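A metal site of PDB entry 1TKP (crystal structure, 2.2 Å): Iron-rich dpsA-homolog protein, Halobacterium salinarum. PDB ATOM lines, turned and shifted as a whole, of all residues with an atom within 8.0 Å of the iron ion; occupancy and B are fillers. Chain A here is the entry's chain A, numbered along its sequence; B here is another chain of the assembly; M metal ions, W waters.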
ATOM      1  N   GLU A  75       4.353  24.933  16.389  1.00  0.00           N
ATOM      2  CA  GLU A  75       3.400  25.312  15.296  1.00  0.00           C
ATOM      3  C   GLU A  75       4.018  25.082  13.923  1.00  0.00           C
ATOM      4  O   GLU A  75       3.387  24.541  12.971  1.00  0.00           O
ATOM      5  CB  GLU A  75       2.961  26.785  15.474  1.00  0.00           C
ATOM      6  CG  GLU A  75       1.757  27.135  14.600  1.00  0.00           C
ATOM      7  CD  GLU A  75       1.634  28.603  14.249  1.00  0.00           C
ATOM      8  OE1 GLU A  75       2.277  29.470  14.966  1.00  0.00           O
ATOM      9  OE2 GLU A  75       0.889  28.899  13.256  1.00  0.00           O
ATOM     10  N   GLU A  76       5.274  25.395  13.818  1.00  0.00           N
ATOM     11  CA  GLU A  76       6.001  25.353  12.570  1.00  0.00           C
ATOM     12  C   GLU A  76       6.305  23.902  12.287  1.00  0.00           C
ATOM     13  O   GLU A  76       6.170  23.438  11.145  1.00  0.00           O
ATOM     14  CB  GLU A  76       7.398  26.005  12.766  1.00  0.00           C
ATOM     15  CG  GLU A  76       7.715  27.386  12.184  1.00  0.00           C
ATOM     16  CD  GLU A  76       8.944  28.102  12.858  1.00  0.00           C
ATOM     17  OE1 GLU A  76      10.167  27.568  12.932  1.00  0.00           O
ATOM     18  OE2 GLU A  76       8.705  29.255  13.268  1.00  0.00           O
ATOM     19  N   ALA A  78       4.421  21.477  13.379  1.00  0.00           N
ATOM     20  CA  ALA A  78       3.203  20.781  12.994  1.00  0.00           C
ATOM     21  C   ALA A  78       2.894  21.132  11.537  1.00  0.00           C
ATOM     22  O   ALA A  78       2.415  20.287  10.743  1.00  0.00           O
ATOM     23  CB  ALA A  78       2.062  21.209  13.823  1.00  0.00           C
ATOM     24  N   ASP A  79       3.044  22.418  11.180  1.00  0.00           N
ATOM     25  CA  ASP A  79       2.814  22.788   9.796  1.00  0.00           C
ATOM     26  C   ASP A  79       3.675  21.952   8.860  1.00  0.00           C
ATOM     27  O   ASP A  79       3.207  21.516   7.834  1.00  0.00           O
ATOM     28  CB  ASP A  79       3.148  24.310   9.609  1.00  0.00           C
ATOM     29  CG  ASP A  79       2.747  24.767   8.269  1.00  0.00           C
ATOM     30  OD1 ASP A  79       1.505  24.804   8.022  1.00  0.00           O
ATOM     31  OD2 ASP A  79       3.585  25.030   7.321  1.00  0.00           O
ATOM     32  N   GLU A  80       4.957  21.751   9.143  1.00  0.00           N
ATOM     33  CA  GLU A  80       5.759  20.861   8.232  1.00  0.00           C
ATOM     34  C   GLU A  80       5.205  19.442   8.057  1.00  0.00           C
ATOM     35  O   GLU A  80       5.163  18.867   6.967  1.00  0.00           O
ATOM     36  CB  GLU A  80       7.237  20.716   8.695  1.00  0.00           C
ATOM     37  CG  GLU A  80       7.911  22.004   8.534  1.00  0.00           C
ATOM     38  CD  GLU A  80       8.375  22.247   7.112  1.00  0.00           C
ATOM     39  OE1 GLU A  80       7.842  23.219   6.441  1.00  0.00           O
ATOM     40  OE2 GLU A  80       9.310  21.497   6.636  1.00  0.00           O
ATOM     41  N   ALA A  82       2.131  18.322   8.750  1.00  0.00           N
ATOM     42  CA  ALA A  82       0.846  18.334   8.028  1.00  0.00           C
ATOM     43  C   ALA A  82       1.075  18.438   6.521  1.00  0.00           C
ATOM     44  O   ALA A  82       0.364  17.804   5.705  1.00  0.00           O
ATOM     45  CB  ALA A  82      -0.070  19.492   8.486  1.00  0.00           C
ATOM     46  N   GLU A  83       1.976  19.332   6.132  1.00  0.00           N
ATOM     47  CA  GLU A  83       2.200  19.603   4.671  1.00  0.00           C
ATOM     48  C   GLU A  83       2.815  18.401   4.071  1.00  0.00           C
ATOM     49  O   GLU A  83       2.457  18.049   2.936  1.00  0.00           O
ATOM     50  CB  GLU A  83       3.085  20.823   4.421  1.00  0.00           C
ATOM     51  CG  GLU A  83       2.214  22.056   4.477  1.00  0.00           C
ATOM     52  CD  GLU A  83       2.912  23.395   4.620  1.00  0.00           C
ATOM     53  OE1 GLU A  83       2.213  24.418   4.934  1.00  0.00           O
ATOM     54  OE2 GLU A  83       4.152  23.470   4.406  1.00  0.00           O
ATOM     55  N   LYS B  49      -5.843  26.395   8.682  1.00  0.00           N
ATOM     56  CA  LYS B  49      -4.656  25.600   8.530  1.00  0.00           C
ATOM     57  C   LYS B  49      -4.973  24.470   7.632  1.00  0.00           C
ATOM     58  O   LYS B  49      -4.213  24.139   6.701  1.00  0.00           O
ATOM     59  CB  LYS B  49      -4.188  24.986   9.860  1.00  0.00           C
ATOM     60  CG  LYS B  49      -3.402  26.003  10.757  1.00  0.00           C
ATOM     61  CD  LYS B  49      -2.314  26.926  10.069  1.00  0.00           C
ATOM     62  CE  LYS B  49      -1.202  26.131   9.483  1.00  0.00           C
ATOM     63  NZ  LYS B  49       0.216  26.840   9.776  1.00  0.00           N
ATOM     64  N   HIS B  52      -5.384  25.748   3.987  1.00  0.00           N
ATOM     65  CA  HIS B  52      -4.010  26.067   3.621  1.00  0.00           C
ATOM     66  C   HIS B  52      -3.237  24.820   3.165  1.00  0.00           C
ATOM     67  O   HIS B  52      -2.511  24.882   2.152  1.00  0.00           O
ATOM     68  CB  HIS B  52      -3.333  26.607   4.906  1.00  0.00           C
ATOM     69  CG  HIS B  52      -1.850  26.798   4.837  1.00  0.00           C
ATOM     70  ND1 HIS B  52      -1.225  27.752   4.052  1.00  0.00           N
ATOM     71  CD2 HIS B  52      -0.851  26.147   5.474  1.00  0.00           C
ATOM     72  CE1 HIS B  52       0.080  27.728   4.283  1.00  0.00           C
ATOM     73  NE2 HIS B  52       0.315  26.805   5.204  1.00  0.00           N
ATOM     74  N   TRP B  53      -3.272  23.741   3.954  1.00  0.00           N
ATOM     75  CA  TRP B  53      -2.535  22.548   3.705  1.00  0.00           C
ATOM     76  C   TRP B  53      -3.049  21.867   2.501  1.00  0.00           C
ATOM     77  O   TRP B  53      -2.257  21.340   1.692  1.00  0.00           O
ATOM     78  CB  TRP B  53      -2.748  21.564   4.844  1.00  0.00           C
ATOM     79  CG  TRP B  53      -2.091  22.022   6.048  1.00  0.00           C
ATOM     80  CD1 TRP B  53      -1.030  22.867   6.112  1.00  0.00           C
ATOM     81  CD2 TRP B  53      -2.423  21.691   7.385  1.00  0.00           C
ATOM     82  NE1 TRP B  53      -0.663  23.075   7.416  1.00  0.00           N
ATOM     83  CE2 TRP B  53      -1.511  22.353   8.215  1.00  0.00           C
ATOM     84  CE3 TRP B  53      -3.392  20.879   7.969  1.00  0.00           C
ATOM     85  CZ2 TRP B  53      -1.576  22.276   9.616  1.00  0.00           C
ATOM     86  CZ3 TRP B  53      -3.402  20.743   9.349  1.00  0.00           C
ATOM     87  CH2 TRP B  53      -2.503  21.437  10.154  1.00  0.00           C
ATOM     88  N   HIS B  64      -3.053  29.345  -0.945  1.00  0.00           N
ATOM     89  CA  HIS B  64      -2.305  28.687   0.064  1.00  0.00           C
ATOM     90  C   HIS B  64      -1.696  29.791   0.906  1.00  0.00           C
ATOM     91  O   HIS B  64      -1.641  29.765   2.160  1.00  0.00           O
ATOM     92  CB  HIS B  64      -1.292  27.782  -0.671  1.00  0.00           C
ATOM     93  CG  HIS B  64      -0.244  27.228   0.189  1.00  0.00           C
ATOM     94  ND1 HIS B  64      -0.430  26.078   0.950  1.00  0.00           N
ATOM     95  CD2 HIS B  64       1.036  27.609   0.377  1.00  0.00           C
ATOM     96  CE1 HIS B  64       0.689  25.814   1.615  1.00  0.00           C
ATOM     97  NE2 HIS B  64       1.589  26.753   1.302  1.00  0.00           N
ATOM     98  N   LEU B  67      -4.386  31.651   2.816  1.00  0.00           N
ATOM     99  CA  LEU B  67      -4.911  30.897   3.943  1.00  0.00           C
ATOM    100  C   LEU B  67      -3.964  30.761   5.115  1.00  0.00           C
ATOM    101  O   LEU B  67      -4.371  30.856   6.245  1.00  0.00           O
ATOM    102  CB  LEU B  67      -5.506  29.588   3.482  1.00  0.00           C
ATOM    103  CG  LEU B  67      -6.792  29.776   2.645  1.00  0.00           C
ATOM    104  CD1 LEU B  67      -6.985  28.426   1.949  1.00  0.00           C
ATOM    105  CD2 LEU B  67      -8.052  30.031   3.511  1.00  0.00           C
ATOM    106  N   GLY B  68      -2.659  30.665   4.811  1.00  0.00           N
ATOM    107  CA  GLY B  68      -1.645  30.663   5.818  1.00  0.00           C
ATOM    108  C   GLY B  68      -1.543  31.988   6.527  1.00  0.00           C
ATOM    109  O   GLY B  68      -1.390  31.962   7.804  1.00  0.00           O
ATOM    110  N   GLU B  69      -1.617  33.102   5.777  1.00  0.00           N
ATOM    111  CA  GLU B  69      -1.694  34.446   6.358  1.00  0.00           C
ATOM    112  C   GLU B  69      -2.960  34.630   7.281  1.00  0.00           C
ATOM    113  O   GLU B  69      -2.825  35.160   8.436  1.00  0.00           O
ATOM    114  CB  GLU B  69      -1.769  35.516   5.276  1.00  0.00           C
ATOM    115  CG  GLU B  69      -0.378  35.900   4.746  1.00  0.00           C
ATOM    116  CD  GLU B  69      -0.394  36.722   3.444  1.00  0.00           C
ATOM    117  OE1 GLU B  69      -1.226  37.688   3.326  1.00  0.00           O
ATOM    118  OE2 GLU B  69       0.464  36.388   2.511  1.00  0.00           O
HETATM  119 FE    FE M   1       2.143  26.105   5.977  1.00  0.00          FE
HETATM  120  O   HOH W   1       3.409  26.968   4.366  1.00  0.00           O
HETATM  121  O   HOH W   2       2.244  28.007   7.171  1.00  0.00           O
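The iron ion is bound by OE1 of Glu 83, NE2 of His 52 of chain B, water W1, OD2 of Asp 79, water W2 and OD1 of Asp 79.
Within 4 Å of the iron ion: Asp 79, Glu 83 and His 52 of chain B.
The backbone carbonyl oxygen (O) of His 52 of chain B sits at hydrogen-bond distance from a ring nitrogen (ND1) of His 64 of chain B (2.7 Å).
The backbone NH (N) of Gly 68 of chain B sits at hydrogen-bond distance from a ring nitrogen (ND1) of His 52 of chain B (3.3 Å).
OD1 of Asp 79 sits close to NZ of Lys 49 of chain B (3.0 Å).
OD1 of Asp 79 sits close to NE1 of Trp 53 of chain B (2.8 Å).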
